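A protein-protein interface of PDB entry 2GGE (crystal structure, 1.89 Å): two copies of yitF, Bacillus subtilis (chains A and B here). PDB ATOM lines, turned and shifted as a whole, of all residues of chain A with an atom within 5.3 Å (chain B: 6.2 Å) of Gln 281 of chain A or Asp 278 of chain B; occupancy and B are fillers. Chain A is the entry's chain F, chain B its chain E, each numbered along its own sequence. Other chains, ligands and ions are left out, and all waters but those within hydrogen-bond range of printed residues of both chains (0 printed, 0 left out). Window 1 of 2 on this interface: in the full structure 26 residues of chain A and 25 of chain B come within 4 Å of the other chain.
Gln 281 of chain A touches Asp 278 of chain B, but with the chains exchanged Asp 278 of chain A does not touch Gln 281 of chain B (4.02 Å).
Leu 282 of chain B touches its own counterpart, Leu 282 of chain A.
Of the 5 pairs that touch across the chains among the printed residues, 1 has its exchanged pair printed and touching as well.
Among the printed residues, merely in contact across the chains: Gln 281 of chain A with Asp 278 of chain B, Leu 282 of chain A with Leu 282 of chain B, Tyr 285 of chain A with Pro 248 of chain B and Tyr 285 of chain A with Glu 275 of chain B.
Of chain B, only Asp 278 (3.6 Å) comes within 4 Å of Gln 281 of chain A.
Asp 278 of chain B touches just these residues of chain A: Gln 281 (3.6 Å) and Tyr 285 (2.6 Å).
Printed residues of chain A within 4 Å of Pro 248 of chain B: Tyr 285 (3.4 Å).
Printed residues of chain A within 4 Å of Leu 282 of chain B: Leu 282 (3.7 Å).
Of the printed residues of chain A, Glu 275 of chain B touches Tyr 285.
Printed residues of chain B within 4 Å of Tyr 285 of chain A: Pro 248 (3.4 Å), Glu 275 (3.6 Å) and Asp 278 (2.6 Å).
Of the printed residues of chain B, Leu 282 of chain A touches Leu 282 (3.7 Å).
Ala 283 of chain B touches none of the printed residues of chain A.
The nearest residue of chain B that does not touch Gln 281 of chain A is Glu 275 of chain B (6.1 Å).
The nearest residue of chain A that does not touch Asp 278 of chain B is Asp 278 of chain A (4.5 Å).
Of the 13 printed residues of chain A, 3 touch a printed residue of chain B.
Printed residues of chain A that touch a printed residue of chain B: Gln 281, Leu 282 and Tyr 285.
Hydrophobic or aromatic side chains of chain A that line the printed part of chain B: Leu 282 and Tyr 285.
Of the 12 printed residues of chain B, 4 touch a printed residue of chain A.
Hydrophobic or aromatic side chains of chain B within 4 Å of the printed part of chain A: Pro 248 and Leu 282.
The side-chain carboxylate (OD2) of Asp 278 of chain B lies within hydrogen-bond range of the side-chain hydroxyl (OH) of Tyr 285 of chain A (2.6 Å).
The backbone carbonyl oxygen (O) of Glu 275 of chain B is in hydrogen-bond range of the side-chain sulfur (SG) of Cys 279 of chain B, at 3.5 Å.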
ATOM      1  N   ARG A 277      21.512  29.589   0.277  1.00  0.00           N
ATOM      2  CA  ARG A 277      22.250  29.598  -0.994  1.00  0.00           C
ATOM      3  C   ARG A 277      23.023  28.278  -1.138  1.00  0.00           C
ATOM      4  O   ARG A 277      23.005  27.669  -2.206  1.00  0.00           O
ATOM      5  CB  ARG A 277      23.188  30.808  -1.059  1.00  0.00           C
ATOM      6  CG  ARG A 277      22.335  32.142  -1.295  1.00  0.00           C
ATOM      7  CD  ARG A 277      23.164  33.292  -1.848  1.00  0.00           C
ATOM      8  NE  ARG A 277      23.711  33.035  -3.178  1.00  0.00           N
ATOM      9  CZ  ARG A 277      25.002  33.081  -3.459  1.00  0.00           C
ATOM     10  NH1 ARG A 277      25.878  33.488  -2.549  1.00  0.00           N
ATOM     11  NH2 ARG A 277      25.396  32.820  -4.694  1.00  0.00           N
ATOM     12  N   ASP A 278      23.669  27.847  -0.062  1.00  0.00           N
ATOM     13  CA  ASP A 278      24.445  26.603  -0.114  1.00  0.00           C
ATOM     14  C   ASP A 278      23.573  25.345  -0.420  1.00  0.00           C
ATOM     15  O   ASP A 278      24.060  24.421  -1.032  1.00  0.00           O
ATOM     16  CB  ASP A 278      25.202  26.388   1.189  1.00  0.00           C
ATOM     17  CG  ASP A 278      26.348  27.405   1.407  1.00  0.00           C
ATOM     18  OD1 ASP A 278      26.758  28.156   0.471  1.00  0.00           O
ATOM     19  OD2 ASP A 278      26.827  27.446   2.546  1.00  0.00           O
ATOM     20  N   CYS A 279      22.342  25.275   0.079  1.00  0.00           N
ATOM     21  CA  CYS A 279      21.338  24.243  -0.390  1.00  0.00           C
ATOM     22  C   CYS A 279      21.144  24.202  -1.910  1.00  0.00           C
ATOM     23  O   CYS A 279      21.284  23.129  -2.546  1.00  0.00           O
ATOM     24  CB  CYS A 279      19.980  24.516   0.260  1.00  0.00           C
ATOM     25  SG  CYS A 279      20.040  24.390   2.037  1.00  0.00           S
ATOM     26  N   LEU A 280      20.852  25.363  -2.500  1.00  0.00           N
ATOM     27  CA  LEU A 280      20.687  25.456  -3.937  1.00  0.00           C
ATOM     28  C   LEU A 280      21.919  24.941  -4.688  1.00  0.00           C
ATOM     29  O   LEU A 280      21.790  24.119  -5.578  1.00  0.00           O
ATOM     30  CB  LEU A 280      20.378  26.919  -4.362  1.00  0.00           C
ATOM     31  CG  LEU A 280      19.122  27.608  -3.800  1.00  0.00           C
ATOM     32  CD1 LEU A 280      19.013  29.052  -4.310  1.00  0.00           C
ATOM     33  CD2 LEU A 280      17.781  26.865  -4.045  1.00  0.00           C
ATOM     34  N   GLN A 281      23.098  25.450  -4.332  1.00  0.00           N
ATOM     35  CA  GLN A 281      24.348  25.060  -4.973  1.00  0.00           C
ATOM     36  C   GLN A 281      24.600  23.518  -4.740  1.00  0.00           C
ATOM     37  O   GLN A 281      25.075  22.823  -5.637  1.00  0.00           O
ATOM     38  CB  GLN A 281      25.484  25.934  -4.384  1.00  0.00           C
ATOM     39  CG  GLN A 281      26.650  26.294  -5.350  1.00  0.00           C
ATOM     40  CD  GLN A 281      26.190  26.945  -6.625  1.00  0.00           C
ATOM     41  OE1 GLN A 281      26.327  26.355  -7.720  1.00  0.00           O
ATOM     42  NE2 GLN A 281      25.570  28.133  -6.502  1.00  0.00           N
ATOM     43  N   LEU A 282      24.332  23.052  -3.525  1.00  0.00           N
ATOM     44  CA  LEU A 282      24.445  21.629  -3.157  1.00  0.00           C
ATOM     45  C   LEU A 282      23.653  20.749  -4.116  1.00  0.00           C
ATOM     46  O   LEU A 282      24.206  19.817  -4.672  1.00  0.00           O
ATOM     47  CB  LEU A 282      23.969  21.401  -1.717  1.00  0.00           C
ATOM     48  CG  LEU A 282      24.040  19.946  -1.257  1.00  0.00           C
ATOM     49  CD1 LEU A 282      25.514  19.654  -1.121  1.00  0.00           C
ATOM     50  CD2 LEU A 282      23.358  19.766   0.088  1.00  0.00           C
ATOM     51  N   ALA A 283      22.391  21.118  -4.372  1.00  0.00           N
ATOM     52  CA  ALA A 283      21.541  20.485  -5.410  1.00  0.00           C
ATOM     53  C   ALA A 283      22.235  20.422  -6.764  1.00  0.00           C
ATOM     54  O   ALA A 283      22.299  19.364  -7.411  1.00  0.00           O
ATOM     55  CB  ALA A 283      20.237  21.218  -5.549  1.00  0.00           C
ATOM     56  N   ARG A 284      22.731  21.567  -7.201  1.00  0.00           N
ATOM     57  CA  ARG A 284      23.473  21.651  -8.477  1.00  0.00           C
ATOM     58  C   ARG A 284      24.671  20.691  -8.506  1.00  0.00           C
ATOM     59  O   ARG A 284      24.862  19.973  -9.489  1.00  0.00           O
ATOM     60  CB  ARG A 284      23.955  23.085  -8.709  1.00  0.00           C
ATOM     61  CG  ARG A 284      22.818  24.021  -9.134  1.00  0.00           C
ATOM     62  CD  ARG A 284      22.499  23.875 -10.614  1.00  0.00           C
ATOM     63  NE  ARG A 284      21.512  24.874 -11.035  1.00  0.00           N
ATOM     64  CZ  ARG A 284      20.193  24.782 -10.828  1.00  0.00           C
ATOM     65  NH1 ARG A 284      19.640  23.716 -10.230  1.00  0.00           N
ATOM     66  NH2 ARG A 284      19.412  25.740 -11.285  1.00  0.00           N
ATOM     67  N   TYR A 285      25.428  20.619  -7.417  1.00  0.00           N
ATOM     68  CA  TYR A 285      26.580  19.737  -7.405  1.00  0.00           C
ATOM     69  C   TYR A 285      26.185  18.253  -7.421  1.00  0.00           C
ATOM     70  O   TYR A 285      26.931  17.394  -7.892  1.00  0.00           O
ATOM     71  CB  TYR A 285      27.458  20.049  -6.211  1.00  0.00           C
ATOM     72  CG  TYR A 285      28.164  21.421  -6.306  1.00  0.00           C
ATOM     73  CD1 TYR A 285      28.717  21.867  -7.518  1.00  0.00           C
ATOM     74  CD2 TYR A 285      28.271  22.244  -5.189  1.00  0.00           C
ATOM     75  CE1 TYR A 285      29.346  23.118  -7.597  1.00  0.00           C
ATOM     76  CE2 TYR A 285      28.896  23.510  -5.251  1.00  0.00           C
ATOM     77  CZ  TYR A 285      29.433  23.938  -6.469  1.00  0.00           C
ATOM     78  OH  TYR A 285      30.109  25.185  -6.563  1.00  0.00           O
ATOM     79  N   PHE A 286      25.023  17.942  -6.888  1.00  0.00           N
ATOM     80  CA  PHE A 286      24.497  16.581  -6.963  1.00  0.00           C
ATOM     81  C   PHE A 286      23.743  16.311  -8.227  1.00  0.00           C
ATOM     82  O   PHE A 286      23.337  15.187  -8.455  1.00  0.00           O
ATOM     83  CB  PHE A 286      23.524  16.371  -5.812  1.00  0.00           C
ATOM     84  CG  PHE A 286      24.137  15.739  -4.611  1.00  0.00           C
ATOM     85  CD1 PHE A 286      24.619  16.509  -3.585  1.00  0.00           C
ATOM     86  CD2 PHE A 286      24.228  14.349  -4.516  1.00  0.00           C
ATOM     87  CE1 PHE A 286      25.149  15.897  -2.433  1.00  0.00           C
ATOM     88  CE2 PHE A 286      24.762  13.757  -3.408  1.00  0.00           C
ATOM     89  CZ  PHE A 286      25.230  14.539  -2.360  1.00  0.00           C
ATOM     90  N   CYS A 310      20.981  34.305  -9.015  1.00  0.00           N
ATOM     91  CA  CYS A 310      22.422  33.994  -8.976  1.00  0.00           C
ATOM     92  C   CYS A 310      22.725  32.499  -9.009  1.00  0.00           C
ATOM     93  O   CYS A 310      23.852  32.100  -8.704  1.00  0.00           O
ATOM     94  CB  CYS A 310      23.066  34.546  -7.692  1.00  0.00           C
ATOM     95  SG  CYS A 310      23.088  36.343  -7.552  1.00  0.00           S
ATOM     96  N   LEU A 311      21.738  31.677  -9.350  1.00  0.00           N
ATOM     97  CA  LEU A 311      21.960  30.244  -9.518  1.00  0.00           C
ATOM     98  C   LEU A 311      22.300  29.949 -10.980  1.00  0.00           C
ATOM     99  O   LEU A 311      21.635  30.482 -11.885  1.00  0.00           O
ATOM    100  CB  LEU A 311      20.695  29.471  -9.066  1.00  0.00           C
ATOM    101  CG  LEU A 311      20.802  27.998  -8.649  1.00  0.00           C
ATOM    102  CD1 LEU A 311      21.881  27.811  -7.476  1.00  0.00           C
ATOM    103  CD2 LEU A 311      19.432  27.446  -8.272  1.00  0.00           C
ATOM    104  N   PRO A 312      23.315  29.076 -11.252  1.00  0.00           N
ATOM    105  CA  PRO A 312      23.489  28.704 -12.661  1.00  0.00           C
ATOM    106  C   PRO A 312      22.369  27.814 -13.210  1.00  0.00           C
ATOM    107  O   PRO A 312      21.607  27.199 -12.425  1.00  0.00           O
ATOM    108  CB  PRO A 312      24.837  27.940 -12.676  1.00  0.00           C
ATOM    109  CG  PRO A 312      25.112  27.573 -11.301  1.00  0.00           C
ATOM    110  CD  PRO A 312      24.319  28.456 -10.372  1.00  0.00           C
ATOM    111  N   PRO B 248      33.541  20.970  -6.529  1.00  0.00           N
ATOM    112  CA  PRO B 248      32.652  20.256  -5.611  1.00  0.00           C
ATOM    113  C   PRO B 248      31.883  19.065  -6.266  1.00  0.00           C
ATOM    114  O   PRO B 248      31.705  18.051  -5.626  1.00  0.00           O
ATOM    115  CB  PRO B 248      31.686  21.335  -5.116  1.00  0.00           C
ATOM    116  CG  PRO B 248      32.354  22.635  -5.402  1.00  0.00           C
ATOM    117  CD  PRO B 248      33.229  22.416  -6.617  1.00  0.00           C
ATOM    118  N   ILE B 273      37.530  30.837  -7.246  1.00  0.00           N
ATOM    119  CA  ILE B 273      37.563  30.977  -5.790  1.00  0.00           C
ATOM    120  C   ILE B 273      36.184  30.677  -5.118  1.00  0.00           C
ATOM    121  O   ILE B 273      36.136  30.107  -4.018  1.00  0.00           O
ATOM    122  CB  ILE B 273      38.200  32.329  -5.333  1.00  0.00           C
ATOM    123  CG1 ILE B 273      38.340  32.362  -3.805  1.00  0.00           C
ATOM    124  CG2 ILE B 273      37.290  33.465  -5.686  1.00  0.00           C
ATOM    125  CD1 ILE B 273      39.388  31.364  -3.230  1.00  0.00           C
ATOM    126  N   ASP B 274      35.087  31.097  -5.735  1.00  0.00           N
ATOM    127  CA  ASP B 274      33.786  30.796  -5.155  1.00  0.00           C
ATOM    128  C   ASP B 274      33.542  29.276  -5.080  1.00  0.00           C
ATOM    129  O   ASP B 274      33.071  28.797  -4.015  1.00  0.00           O
ATOM    130  CB  ASP B 274      32.631  31.549  -5.853  1.00  0.00           C
ATOM    131  CG  ASP B 274      32.866  33.068  -5.883  1.00  0.00           C
ATOM    132  OD1 ASP B 274      33.000  33.669  -4.764  1.00  0.00           O
ATOM    133  OD2 ASP B 274      32.970  33.656  -7.007  1.00  0.00           O
ATOM    134  N   GLU B 275      33.912  28.562  -6.150  1.00  0.00           N
ATOM    135  CA  GLU B 275      33.806  27.108  -6.221  1.00  0.00           C
ATOM    136  C   GLU B 275      34.742  26.442  -5.196  1.00  0.00           C
ATOM    137  O   GLU B 275      34.367  25.439  -4.597  1.00  0.00           O
ATOM    138  CB  GLU B 275      33.993  26.531  -7.641  1.00  0.00           C
ATOM    139  CG  GLU B 275      32.711  26.688  -8.522  1.00  0.00           C
ATOM    140  CD  GLU B 275      32.405  25.586  -9.632  1.00  0.00           C
ATOM    141  OE1 GLU B 275      32.809  24.369  -9.598  1.00  0.00           O
ATOM    142  OE2 GLU B 275      31.653  25.968 -10.575  1.00  0.00           O
ATOM    143  N   PHE B 276      35.917  27.042  -4.963  1.00  0.00           N
ATOM    144  CA  PHE B 276      36.844  26.565  -3.944  1.00  0.00           C
ATOM    145  C   PHE B 276      36.245  26.669  -2.563  1.00  0.00           C
ATOM    146  O   PHE B 276      36.410  25.745  -1.789  1.00  0.00           O
ATOM    147  CB  PHE B 276      38.127  27.365  -3.973  1.00  0.00           C
ATOM    148  CG  PHE B 276      39.072  27.009  -2.905  1.00  0.00           C
ATOM    149  CD1 PHE B 276      40.041  26.022  -3.129  1.00  0.00           C
ATOM    150  CD2 PHE B 276      39.013  27.625  -1.662  1.00  0.00           C
ATOM    151  CE1 PHE B 276      40.974  25.707  -2.126  1.00  0.00           C
ATOM    152  CE2 PHE B 276      39.910  27.290  -0.673  1.00  0.00           C
ATOM    153  CZ  PHE B 276      40.882  26.308  -0.890  1.00  0.00           C
ATOM    154  N   ARG B 277      35.601  27.801  -2.220  1.00  0.00           N
ATOM    155  CA  ARG B 277      34.921  27.930  -0.942  1.00  0.00           C
ATOM    156  C   ARG B 277      33.766  26.886  -0.783  1.00  0.00           C
ATOM    157  O   ARG B 277      33.534  26.344   0.347  1.00  0.00           O
ATOM    158  CB  ARG B 277      34.388  29.340  -0.718  1.00  0.00           C
ATOM    159  CG  ARG B 277      35.450  30.464  -0.719  1.00  0.00           C
ATOM    160  CD  ARG B 277      34.847  31.776  -0.214  1.00  0.00           C
ATOM    161  NE  ARG B 277      34.415  31.734   1.184  1.00  0.00           N
ATOM    162  CZ  ARG B 277      33.227  32.127   1.627  1.00  0.00           C
ATOM    163  NH1 ARG B 277      32.339  32.697   0.795  1.00  0.00           N
ATOM    164  NH2 ARG B 277      32.944  31.993   2.920  1.00  0.00           N
ATOM    165  N   ASP B 278      33.114  26.554  -1.904  1.00  0.00           N
ATOM    166  CA  ASP B 278      32.009  25.518  -1.917  1.00  0.00           C
ATOM    167  C   ASP B 278      32.562  24.146  -1.627  1.00  0.00           C
ATOM    168  O   ASP B 278      31.951  23.372  -0.831  1.00  0.00           O
ATOM    169  CB  ASP B 278      31.281  25.461  -3.230  1.00  0.00           C
ATOM    170  CG  ASP B 278      30.407  26.725  -3.491  1.00  0.00           C
ATOM    171  OD1 ASP B 278      30.007  27.416  -2.536  1.00  0.00           O
ATOM    172  OD2 ASP B 278      30.126  27.013  -4.669  1.00  0.00           O
ATOM    173  N   CYS B 279      33.753  23.845  -2.174  1.00  0.00           N
ATOM    174  CA  CYS B 279      34.447  22.607  -1.714  1.00  0.00           C
ATOM    175  C   CYS B 279      34.625  22.537  -0.186  1.00  0.00           C
ATOM    176  O   CYS B 279      34.373  21.500   0.427  1.00  0.00           O
ATOM    177  CB  CYS B 279      35.807  22.399  -2.356  1.00  0.00           C
ATOM    178  SG  CYS B 279      35.788  22.262  -4.123  1.00  0.00           S
ATOM    179  N   LEU B 280      35.127  23.614   0.430  1.00  0.00           N
ATOM    180  CA  LEU B 280      35.333  23.629   1.872  1.00  0.00           C
ATOM    181  C   LEU B 280      34.040  23.435   2.667  1.00  0.00           C
ATOM    182  O   LEU B 280      34.029  22.661   3.606  1.00  0.00           O
ATOM    183  CB  LEU B 280      36.036  24.938   2.299  1.00  0.00           C
ATOM    184  CG  LEU B 280      37.421  25.285   1.682  1.00  0.00           C
ATOM    185  CD1 LEU B 280      38.002  26.450   2.349  1.00  0.00           C
ATOM    186  CD2 LEU B 280      38.475  24.119   1.771  1.00  0.00           C
ATOM    187  N   GLN B 281      32.978  24.162   2.325  1.00  0.00           N
ATOM    188  CA  GLN B 281      31.663  24.053   3.011  1.00  0.00           C
ATOM    189  C   GLN B 281      31.033  22.671   2.749  1.00  0.00           C
ATOM    190  O   GLN B 281      30.376  22.127   3.634  1.00  0.00           O
ATOM    191  CB  GLN B 281      30.643  25.070   2.473  1.00  0.00           C
ATOM    192  CG  GLN B 281      30.714  26.493   2.958  1.00  0.00           C
ATOM    193  CD  GLN B 281      30.676  26.679   4.496  1.00  0.00           C
ATOM    194  OE1 GLN B 281      29.863  26.079   5.225  1.00  0.00           O
ATOM    195  NE2 GLN B 281      31.559  27.550   4.975  1.00  0.00           N
ATOM    196  N   LEU B 282      31.224  22.132   1.538  1.00  0.00           N
ATOM    197  CA  LEU B 282      30.740  20.718   1.208  1.00  0.00           C
ATOM    198  C   LEU B 282      31.322  19.702   2.204  1.00  0.00           C
ATOM    199  O   LEU B 282      30.648  18.791   2.706  1.00  0.00           O
ATOM    200  CB  LEU B 282      31.152  20.364  -0.209  1.00  0.00           C
ATOM    201  CG  LEU B 282      30.721  19.041  -0.799  1.00  0.00           C
ATOM    202  CD1 LEU B 282      29.220  19.143  -1.133  1.00  0.00           C
ATOM    203  CD2 LEU B 282      31.556  18.672  -1.980  1.00  0.00           C
ATOM    204  N   ALA B 283      32.598  19.883   2.505  1.00  0.00           N
ATOM    205  CA  ALA B 283      33.275  19.023   3.422  1.00  0.00           C
ATOM    206  C   ALA B 283      32.609  19.207   4.804  1.00  0.00           C
ATOM    207  O   ALA B 283      32.253  18.245   5.493  1.00  0.00           O
ATOM    208  CB  ALA B 283      34.711  19.435   3.467  1.00  0.00           C
